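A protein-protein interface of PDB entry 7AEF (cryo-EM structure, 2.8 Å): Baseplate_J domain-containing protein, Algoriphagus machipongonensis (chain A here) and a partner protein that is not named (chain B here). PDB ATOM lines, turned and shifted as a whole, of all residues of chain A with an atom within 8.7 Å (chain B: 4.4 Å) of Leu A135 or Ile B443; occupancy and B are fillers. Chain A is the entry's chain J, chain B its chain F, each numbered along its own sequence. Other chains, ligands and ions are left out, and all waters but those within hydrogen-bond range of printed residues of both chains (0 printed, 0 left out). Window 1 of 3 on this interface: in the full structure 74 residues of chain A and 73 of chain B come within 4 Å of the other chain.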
ATOM      1  N   PRO A  29     -14.504  -2.618  13.544  1.00  0.00           N
ATOM      2  CA  PRO A  29     -15.839  -2.502  14.155  1.00  0.00           C
ATOM      3  C   PRO A  29     -16.802  -3.616  13.832  1.00  0.00           C
ATOM      4  O   PRO A  29     -17.560  -4.031  14.715  1.00  0.00           O
ATOM      5  CB  PRO A  29     -16.332  -1.177  13.573  1.00  0.00           C
ATOM      6  CG  PRO A  29     -15.089  -0.395  13.360  1.00  0.00           C
ATOM      7  CD  PRO A  29     -14.065  -1.362  12.922  1.00  0.00           C
ATOM      8  N   VAL A  32     -18.295  -6.731  15.965  1.00  0.00           N
ATOM      9  CA  VAL A  32     -19.350  -6.592  16.943  1.00  0.00           C
ATOM     10  C   VAL A  32     -20.668  -6.317  16.249  1.00  0.00           C
ATOM     11  O   VAL A  32     -20.830  -5.290  15.580  1.00  0.00           O
ATOM     12  CB  VAL A  32     -19.030  -5.472  17.927  1.00  0.00           C
ATOM     13  CG1 VAL A  32     -20.159  -5.323  18.930  1.00  0.00           C
ATOM     14  CG2 VAL A  32     -17.738  -5.772  18.602  1.00  0.00           C
ATOM     15  N   LEU A  34     -24.223  -5.486  17.314  1.00  0.00           N
ATOM     16  CA  LEU A  34     -24.993  -5.094  18.488  1.00  0.00           C
ATOM     17  C   LEU A  34     -26.338  -5.792  18.547  1.00  0.00           C
ATOM     18  O   LEU A  34     -26.816  -6.139  19.627  1.00  0.00           O
ATOM     19  CB  LEU A  34     -25.217  -3.593  18.493  1.00  0.00           C
ATOM     20  CG  LEU A  34     -24.008  -2.696  18.656  1.00  0.00           C
ATOM     21  CD1 LEU A  34     -24.453  -1.275  18.426  1.00  0.00           C
ATOM     22  CD2 LEU A  34     -23.415  -2.859  20.029  1.00  0.00           C
ATOM     23  N   GLN A  35     -26.947  -6.033  17.400  1.00  0.00           N
ATOM     24  CA  GLN A  35     -28.227  -6.719  17.307  1.00  0.00           C
ATOM     25  C   GLN A  35     -28.071  -7.911  16.379  1.00  0.00           C
ATOM     26  O   GLN A  35     -27.742  -7.709  15.223  1.00  0.00           O
ATOM     27  CB  GLN A  35     -29.248  -5.760  16.715  1.00  0.00           C
ATOM     28  CG  GLN A  35     -30.647  -6.286  16.657  1.00  0.00           C
ATOM     29  CD  GLN A  35     -31.367  -6.060  17.950  1.00  0.00           C
ATOM     30  OE1 GLN A  35     -31.366  -4.957  18.487  1.00  0.00           O
ATOM     31  NE2 GLN A  35     -31.974  -7.108  18.473  1.00  0.00           N
ATOM     32  N   SER A 128     -33.677  -1.849   9.766  1.00  0.00           N
ATOM     33  CA  SER A 128     -33.338  -1.169  10.996  1.00  0.00           C
ATOM     34  C   SER A 128     -32.112  -1.791  11.602  1.00  0.00           C
ATOM     35  O   SER A 128     -31.267  -1.090  12.154  1.00  0.00           O
ATOM     36  CB  SER A 128     -34.501  -1.223  11.973  1.00  0.00           C
ATOM     37  OG  SER A 128     -35.599  -0.512  11.462  1.00  0.00           O
ATOM     38  N   LYS A 129     -32.006  -3.103  11.467  1.00  0.00           N
ATOM     39  CA  LYS A 129     -30.849  -3.815  11.944  1.00  0.00           C
ATOM     40  C   LYS A 129     -29.607  -3.329  11.230  1.00  0.00           C
ATOM     41  O   LYS A 129     -28.582  -3.110  11.854  1.00  0.00           O
ATOM     42  CB  LYS A 129     -31.083  -5.297  11.713  1.00  0.00           C
ATOM     43  CG  LYS A 129     -30.027  -6.221  12.242  1.00  0.00           C
ATOM     44  CD  LYS A 129     -30.431  -7.650  11.984  1.00  0.00           C
ATOM     45  CE  LYS A 129     -29.270  -8.584  12.184  1.00  0.00           C
ATOM     46  NZ  LYS A 129     -29.494  -9.896  11.536  1.00  0.00           N
ATOM     47  N   LYS A 130     -29.709  -3.091   9.927  1.00  0.00           N
ATOM     48  CA  LYS A 130     -28.573  -2.626   9.146  1.00  0.00           C
ATOM     49  C   LYS A 130     -28.060  -1.282   9.633  1.00  0.00           C
ATOM     50  O   LYS A 130     -26.852  -1.097   9.786  1.00  0.00           O
ATOM     51  CB  LYS A 130     -28.965  -2.531   7.682  1.00  0.00           C
ATOM     52  CG  LYS A 130     -27.831  -2.082   6.796  1.00  0.00           C
ATOM     53  CD  LYS A 130     -28.241  -2.050   5.353  1.00  0.00           C
ATOM     54  CE  LYS A 130     -27.108  -1.556   4.479  1.00  0.00           C
ATOM     55  NZ  LYS A 130     -27.497  -1.518   3.044  1.00  0.00           N
ATOM     56  N   ARG A 131     -28.964  -0.346   9.907  1.00  0.00           N
ATOM     57  CA  ARG A 131     -28.570   0.971  10.397  1.00  0.00           C
ATOM     58  C   ARG A 131     -28.046   0.916  11.822  1.00  0.00           C
ATOM     59  O   ARG A 131     -27.053   1.567  12.152  1.00  0.00           O
ATOM     60  CB  ARG A 131     -29.760   1.913  10.325  1.00  0.00           C
ATOM     61  CG  ARG A 131     -29.438   3.328  10.690  1.00  0.00           C
ATOM     62  CD  ARG A 131     -30.641   4.205  10.570  1.00  0.00           C
ATOM     63  NE  ARG A 131     -31.135   4.271   9.201  1.00  0.00           N
ATOM     64  CZ  ARG A 131     -30.666   5.079   8.255  1.00  0.00           C
ATOM     65  NH1 ARG A 131     -29.669   5.913   8.500  1.00  0.00           N
ATOM     66  NH2 ARG A 131     -31.199   5.049   7.048  1.00  0.00           N
ATOM     67  N   PHE A 132     -28.734   0.183  12.680  1.00  0.00           N
ATOM     68  CA  PHE A 132     -28.391   0.092  14.088  1.00  0.00           C
ATOM     69  C   PHE A 132     -27.011  -0.492  14.313  1.00  0.00           C
ATOM     70  O   PHE A 132     -26.299  -0.053  15.203  1.00  0.00           O
ATOM     71  CB  PHE A 132     -29.435  -0.772  14.766  1.00  0.00           C
ATOM     72  CG  PHE A 132     -29.437  -0.694  16.243  1.00  0.00           C
ATOM     73  CD1 PHE A 132     -30.358   0.073  16.898  1.00  0.00           C
ATOM     74  CD2 PHE A 132     -28.560  -1.436  16.985  1.00  0.00           C
ATOM     75  CE1 PHE A 132     -30.379   0.122  18.266  1.00  0.00           C
ATOM     76  CE2 PHE A 132     -28.565  -1.378  18.343  1.00  0.00           C
ATOM     77  CZ  PHE A 132     -29.478  -0.598  18.984  1.00  0.00           C
ATOM     78  N   ASN A 133     -26.630  -1.499  13.556  1.00  0.00           N
ATOM     79  CA  ASN A 133     -25.329  -2.114  13.767  1.00  0.00           C
ATOM     80  C   ASN A 133     -24.158  -1.294  13.233  1.00  0.00           C
ATOM     81  O   ASN A 133     -23.020  -1.742  13.356  1.00  0.00           O
ATOM     82  CB  ASN A 133     -25.317  -3.508  13.152  1.00  0.00           C
ATOM     83  CG  ASN A 133     -26.021  -4.519  14.019  1.00  0.00           C
ATOM     84  OD1 ASN A 133     -26.087  -4.374  15.236  1.00  0.00           O
ATOM     85  ND2 ASN A 133     -26.551  -5.548  13.403  1.00  0.00           N
ATOM     86  N   GLN A 134     -24.376  -0.111  12.669  1.00  0.00           N
ATOM     87  CA  GLN A 134     -23.261   0.726  12.254  1.00  0.00           C
ATOM     88  C   GLN A 134     -22.808   1.670  13.349  1.00  0.00           C
ATOM     89  O   GLN A 134     -21.860   2.430  13.147  1.00  0.00           O
ATOM     90  CB  GLN A 134     -23.635   1.501  11.002  1.00  0.00           C
ATOM     91  CG  GLN A 134     -23.829   0.592   9.842  1.00  0.00           C
ATOM     92  CD  GLN A 134     -24.324   1.295   8.626  1.00  0.00           C
ATOM     93  OE1 GLN A 134     -23.654   2.157   8.064  1.00  0.00           O
ATOM     94  NE2 GLN A 134     -25.512   0.931   8.202  1.00  0.00           N
ATOM     95  N   LEU A 135     -23.452   1.607  14.510  1.00  0.00           N
ATOM     96  CA  LEU A 135     -23.109   2.477  15.623  1.00  0.00           C
ATOM     97  C   LEU A 135     -21.711   2.230  16.161  1.00  0.00           C
ATOM     98  O   LEU A 135     -21.074   3.174  16.634  1.00  0.00           O
ATOM     99  CB  LEU A 135     -24.115   2.294  16.746  1.00  0.00           C
ATOM    100  CG  LEU A 135     -25.506   2.865  16.530  1.00  0.00           C
ATOM    101  CD1 LEU A 135     -26.422   2.346  17.608  1.00  0.00           C
ATOM    102  CD2 LEU A 135     -25.467   4.369  16.542  1.00  0.00           C
ATOM    103  N   THR A 136     -21.216   0.990  16.109  1.00  0.00           N
ATOM    104  CA  THR A 136     -19.895   0.706  16.658  1.00  0.00           C
ATOM    105  C   THR A 136     -18.811   1.403  15.844  1.00  0.00           C
ATOM    106  O   THR A 136     -17.798   1.829  16.401  1.00  0.00           O
ATOM    107  CB  THR A 136     -19.596  -0.785  16.647  1.00  0.00           C
ATOM    108  OG1 THR A 136     -19.706  -1.279  15.313  1.00  0.00           O
ATOM    109  CG2 THR A 136     -20.608  -1.507  17.496  1.00  0.00           C
ATOM    110  N   LYS A 137     -19.018   1.531  14.534  1.00  0.00           N
ATOM    111  CA  LYS A 137     -18.037   2.217  13.715  1.00  0.00           C
ATOM    112  C   LYS A 137     -18.091   3.704  13.956  1.00  0.00           C
ATOM    113  O   LYS A 137     -17.047   4.347  14.078  1.00  0.00           O
ATOM    114  CB  LYS A 137     -18.249   1.930  12.234  1.00  0.00           C
ATOM    115  CG  LYS A 137     -17.213   2.618  11.360  1.00  0.00           C
ATOM    116  CD  LYS A 137     -17.293   2.198   9.918  1.00  0.00           C
ATOM    117  CE  LYS A 137     -16.278   2.960   9.084  1.00  0.00           C
ATOM    118  NZ  LYS A 137     -16.300   2.570   7.651  1.00  0.00           N
ATOM    119  N   ARG A 138     -19.300   4.257  14.037  1.00  0.00           N
ATOM    120  CA  ARG A 138     -19.457   5.685  14.263  1.00  0.00           C
ATOM    121  C   ARG A 138     -18.830   6.104  15.576  1.00  0.00           C
ATOM    122  O   ARG A 138     -18.197   7.159  15.658  1.00  0.00           O
ATOM    123  CB  ARG A 138     -20.931   6.049  14.256  1.00  0.00           C
ATOM    124  CG  ARG A 138     -21.560   5.959  12.903  1.00  0.00           C
ATOM    125  CD  ARG A 138     -23.045   6.092  12.987  1.00  0.00           C
ATOM    126  NE  ARG A 138     -23.441   7.398  13.483  1.00  0.00           N
ATOM    127  CZ  ARG A 138     -24.661   7.699  13.908  1.00  0.00           C
ATOM    128  NH1 ARG A 138     -25.615   6.787  13.898  1.00  0.00           N
ATOM    129  NH2 ARG A 138     -24.928   8.915  14.343  1.00  0.00           N
ATOM    130  N   HIS A 139     -18.972   5.258  16.591  1.00  0.00           N
ATOM    131  CA  HIS A 139     -18.391   5.503  17.898  1.00  0.00           C
ATOM    132  C   HIS A 139     -16.877   5.545  17.831  1.00  0.00           C
ATOM    133  O   HIS A 139     -16.257   6.479  18.345  1.00  0.00           O
ATOM    134  CB  HIS A 139     -18.857   4.416  18.848  1.00  0.00           C
ATOM    135  CG  HIS A 139     -18.416   4.613  20.252  1.00  0.00           C
ATOM    136  ND1 HIS A 139     -19.031   5.498  21.103  1.00  0.00           N
ATOM    137  CD2 HIS A 139     -17.428   4.028  20.964  1.00  0.00           C
ATOM    138  CE1 HIS A 139     -18.440   5.452  22.281  1.00  0.00           C
ATOM    139  NE2 HIS A 139     -17.463   4.569  22.222  1.00  0.00           N
ATOM    140  N   LEU A 140     -16.267   4.552  17.178  1.00  0.00           N
ATOM    141  CA  LEU A 140     -14.813   4.511  17.064  1.00  0.00           C
ATOM    142  C   LEU A 140     -14.268   5.713  16.318  1.00  0.00           C
ATOM    143  O   LEU A 140     -13.298   6.325  16.767  1.00  0.00           O
ATOM    144  CB  LEU A 140     -14.345   3.240  16.362  1.00  0.00           C
ATOM    145  CG  LEU A 140     -12.831   3.126  16.101  1.00  0.00           C
ATOM    146  CD1 LEU A 140     -12.058   3.130  17.391  1.00  0.00           C
ATOM    147  CD2 LEU A 140     -12.529   1.870  15.323  1.00  0.00           C
ATOM    148  N   ASP A 141     -14.869   6.059  15.174  1.00  0.00           N
ATOM    149  CA  ASP A 141     -14.374   7.184  14.389  1.00  0.00           C
ATOM    150  C   ASP A 141     -14.471   8.476  15.166  1.00  0.00           C
ATOM    151  O   ASP A 141     -13.539   9.279  15.135  1.00  0.00           O
ATOM    152  CB  ASP A 141     -15.143   7.306  13.074  1.00  0.00           C
ATOM    153  CG  ASP A 141     -14.804   6.191  12.098  1.00  0.00           C
ATOM    154  OD1 ASP A 141     -13.788   5.505  12.316  1.00  0.00           O
ATOM    155  OD2 ASP A 141     -15.506   5.947  11.096  1.00  0.00           O
ATOM    156  N   PHE A 142     -15.564   8.663  15.900  1.00  0.00           N
ATOM    157  CA  PHE A 142     -15.727   9.857  16.713  1.00  0.00           C
ATOM    158  C   PHE A 142     -14.584  10.011  17.692  1.00  0.00           C
ATOM    159  O   PHE A 142     -13.930  11.057  17.724  1.00  0.00           O
ATOM    160  CB  PHE A 142     -17.044   9.780  17.449  1.00  0.00           C
ATOM    161  CG  PHE A 142     -17.249  10.864  18.404  1.00  0.00           C
ATOM    162  CD1 PHE A 142     -17.624  12.101  17.972  1.00  0.00           C
ATOM    163  CD2 PHE A 142     -17.109  10.642  19.748  1.00  0.00           C
ATOM    164  CE1 PHE A 142     -17.832  13.095  18.858  1.00  0.00           C
ATOM    165  CE2 PHE A 142     -17.317  11.637  20.627  1.00  0.00           C
ATOM    166  CZ  PHE A 142     -17.679  12.867  20.181  1.00  0.00           C
ATOM    167  N   ILE B  72     -24.105  11.200  17.339  1.00  0.00           N
ATOM    168  CA  ILE B  72     -23.493  10.534  18.487  1.00  0.00           C
ATOM    169  C   ILE B  72     -23.345  11.464  19.661  1.00  0.00           C
ATOM    170  O   ILE B  72     -23.587  11.058  20.803  1.00  0.00           O
ATOM    171  CB  ILE B  72     -22.127   9.945  18.107  1.00  0.00           C
ATOM    172  CG1 ILE B  72     -22.285   8.817  17.071  1.00  0.00           C
ATOM    173  CG2 ILE B  72     -21.392   9.450  19.349  1.00  0.00           C
ATOM    174  CD1 ILE B  72     -23.082   7.591  17.513  1.00  0.00           C
ATOM    175  N   ILE B  76     -25.020   9.579  23.150  1.00  0.00           N
ATOM    176  CA  ILE B  76     -24.284   9.053  24.289  1.00  0.00           C
ATOM    177  C   ILE B  76     -23.973  10.117  25.327  1.00  0.00           C
ATOM    178  O   ILE B  76     -23.057   9.941  26.125  1.00  0.00           O
ATOM    179  CB  ILE B  76     -22.993   8.353  23.870  1.00  0.00           C
ATOM    180  CG1 ILE B  76     -22.092   9.344  23.148  1.00  0.00           C
ATOM    181  CG2 ILE B  76     -23.332   7.143  23.022  1.00  0.00           C
ATOM    182  CD1 ILE B  76     -20.709   8.892  22.961  1.00  0.00           C
ATOM    183  N   HIS B 439     -33.633  -0.336  23.057  1.00  0.00           N
ATOM    184  CA  HIS B 439     -32.265  -0.680  22.741  1.00  0.00           C
ATOM    185  C   HIS B 439     -31.414   0.548  22.472  1.00  0.00           C
ATOM    186  O   HIS B 439     -30.237   0.516  22.775  1.00  0.00           O
ATOM    187  CB  HIS B 439     -32.243  -1.620  21.547  1.00  0.00           C
ATOM    188  CG  HIS B 439     -31.064  -2.541  21.512  1.00  0.00           C
ATOM    189  ND1 HIS B 439     -31.163  -3.839  21.068  1.00  0.00           N
ATOM    190  CD2 HIS B 439     -29.762  -2.350  21.827  1.00  0.00           C
ATOM    191  CE1 HIS B 439     -29.977  -4.412  21.126  1.00  0.00           C
ATOM    192  NE2 HIS B 439     -29.109  -3.529  21.583  1.00  0.00           N
ATOM    193  N   LEU B 440     -31.953   1.613  21.858  1.00  0.00           N
ATOM    194  CA  LEU B 440     -31.172   2.855  21.686  1.00  0.00           C
ATOM    195  C   LEU B 440     -30.772   3.466  23.014  1.00  0.00           C
ATOM    196  O   LEU B 440     -29.653   3.964  23.163  1.00  0.00           O
ATOM    197  CB  LEU B 440     -31.951   3.936  20.946  1.00  0.00           C
ATOM    198  CG  LEU B 440     -32.196   3.842  19.464  1.00  0.00           C
ATOM    199  CD1 LEU B 440     -33.188   4.930  19.061  1.00  0.00           C
ATOM    200  CD2 LEU B 440     -30.886   4.037  18.722  1.00  0.00           C
ATOM    201  N   SER B 441     -31.668   3.424  23.993  1.00  0.00           N
ATOM    202  CA  SER B 441     -31.390   3.998  25.305  1.00  0.00           C
ATOM    203  C   SER B 441     -30.244   3.321  26.044  1.00  0.00           C
ATOM    204  O   SER B 441     -29.768   3.855  27.051  1.00  0.00           O
ATOM    205  CB  SER B 441     -32.608   3.909  26.203  1.00  0.00           C
ATOM    206  OG  SER B 441     -33.638   4.735  25.760  1.00  0.00           O
ATOM    207  N   LYS B 442     -29.825   2.143  25.610  1.00  0.00           N
ATOM    208  CA  LYS B 442     -28.788   1.400  26.287  1.00  0.00           C
ATOM    209  C   LYS B 442     -27.442   1.440  25.591  1.00  0.00           C
ATOM    210  O   LYS B 442     -26.514   0.803  26.092  1.00  0.00           O
ATOM    211  CB  LYS B 442     -29.224  -0.048  26.452  1.00  0.00           C
ATOM    212  CG  LYS B 442     -30.493  -0.234  27.247  1.00  0.00           C
ATOM    213  CD  LYS B 442     -30.345   0.157  28.682  1.00  0.00           C
ATOM    214  CE  LYS B 442     -31.589  -0.212  29.434  1.00  0.00           C
ATOM    215  NZ  LYS B 442     -31.530   0.192  30.862  1.00  0.00           N
ATOM    216  N   ILE B 443     -27.282   2.197  24.501  1.00  0.00           N
ATOM    217  CA  ILE B 443     -25.995   2.163  23.799  1.00  0.00           C
ATOM    218  C   ILE B 443     -24.864   2.599  24.710  1.00  0.00           C
ATOM    219  O   ILE B 443     -23.787   1.990  24.714  1.00  0.00           O
ATOM    220  CB  ILE B 443     -25.994   3.025  22.530  1.00  0.00           C
ATOM    221  CG1 ILE B 443     -26.998   2.489  21.501  1.00  0.00           C
ATOM    222  CG2 ILE B 443     -24.570   3.101  21.935  1.00  0.00           C
ATOM    223  CD1 ILE B 443     -26.797   1.062  21.009  1.00  0.00           C
ATOM    224  N   LYS B 444     -25.121   3.605  25.538  1.00  0.00           N
ATOM    225  CA  LYS B 444     -24.123   4.091  26.478  1.00  0.00           C
ATOM    226  C   LYS B 444     -23.628   3.026  27.423  1.00  0.00           C
ATOM    227  O   LYS B 444     -22.476   3.077  27.855  1.00  0.00           O
ATOM    228  CB  LYS B 444     -24.700   5.162  27.360  1.00  0.00           C
ATOM    229  CG  LYS B 444     -24.928   6.424  26.723  1.00  0.00           C
ATOM    230  CD  LYS B 444     -25.637   7.353  27.665  1.00  0.00           C
ATOM    231  CE  LYS B 444     -24.718   7.842  28.740  1.00  0.00           C
ATOM    232  NZ  LYS B 444     -25.380   8.804  29.595  1.00  0.00           N
ATOM    233  N   SER B 445     -24.510   2.132  27.843  1.00  0.00           N
ATOM    234  CA  SER B 445     -24.111   1.091  28.762  1.00  0.00           C
ATOM    235  C   SER B 445     -23.351   0.012  28.062  1.00  0.00           C
ATOM    236  O   SER B 445     -22.320  -0.443  28.558  1.00  0.00           O
ATOM    237  CB  SER B 445     -25.312   0.504  29.482  1.00  0.00           C
ATOM    238  OG  SER B 445     -26.012   1.474  30.206  1.00  0.00           O
ATOM    239  N   LEU B 446     -23.818  -0.360  26.884  1.00  0.00           N
ATOM    240  CA  LEU B 446     -23.223  -1.475  26.169  1.00  0.00           C
ATOM    241  C   LEU B 446     -21.759  -1.231  25.860  1.00  0.00           C
ATOM    242  O   LEU B 446     -20.944  -2.152  25.942  1.00  0.00           O
ATOM    243  CB  LEU B 446     -23.996  -1.714  24.882  1.00  0.00           C
ATOM    244  CG  LEU B 446     -25.414  -2.275  25.047  1.00  0.00           C
ATOM    245  CD1 LEU B 446     -26.129  -2.181  23.738  1.00  0.00           C
ATOM    246  CD2 LEU B 446     -25.374  -3.730  25.499  1.00  0.00           C
ATOM    247  N   LEU B 447     -21.397   0.014  25.582  1.00  0.00           N
ATOM    248  CA  LEU B 447     -20.023   0.353  25.262  1.00  0.00           C
ATOM    249  C   LEU B 447     -19.276   1.081  26.386  1.00  0.00           C
ATOM    250  O   LEU B 447     -18.238   1.688  26.120  1.00  0.00           O
ATOM    251  CB  LEU B 447     -20.008   1.187  23.988  1.00  0.00           C
ATOM    252  CG  LEU B 447     -20.575   0.496  22.737  1.00  0.00           C
ATOM    253  CD1 LEU B 447     -20.597   1.476  21.613  1.00  0.00           C
ATOM    254  CD2 LEU B 447     -19.740  -0.730  22.353  1.00  0.00           C
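ND1 of His B439 lies within hydrogen-bond range of OE1 of Gln A35 (2.8 Å).
CE1 of His B439 touches O of Leu A34, at 3.9 Å.
CD2 of His B439 touches CZ of Phe A132 (3.4 Å).
Leu B440 touches Phe A132.
CZ of Phe A132 touches CD1 of Ile B443, 3.7 Å away.
CD1 of Leu A135 touches CD1 of Ile B443, at 3.7 Å.
Arg A138 touches Ile B72 (NH2 to CG1, 3.8 Å).
The backbone NH (N) of Leu A34 sits at hydrogen-bond distance from the side-chain amide oxygen (OD1) of Asn A133 (3.0 Å).
The backbone NH (N) of Gln A35 sits at hydrogen-bond distance from the side-chain amide oxygen (OD1) of Asn A133 (2.9 Å).
Of the printed residues of chain B, Leu A135 touches Ile B443.
Of chain A, only Phe A132 and Leu A135 come within 4 Å of Ile B443.
Printed residues of chain B within 4 Å of Leu A34: His B439.
Of the printed residues of chain B, Arg A138 touches Ile B72.
Of the printed residues of chain A, His B439 touches Leu A34 (3.9 Å), Gln A35 (2.8 Å) and Phe A132 (3.4 Å).
Phe A142 touches none of the printed residues of chain B.
The nearest residue of chain A that does not touch Ile B443 is Leu A34 (4.2 Å).
Printed residues of chain B that touch a printed residue of chain A: Ile B72, His B439, Leu B440 and Ile B443.
Of the 19 printed residues of chain A, 5 touch a printed residue of chain B.
Along chain A the printed residues that touch a printed residue of chain B span positions 34 to 138.
Among the printed residues, 7 pairs touch across the chains.
Among the printed residues, no Asp or Glu carboxylate lies within 4 Å of a Lys or Arg side-chain nitrogen of the other chain.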
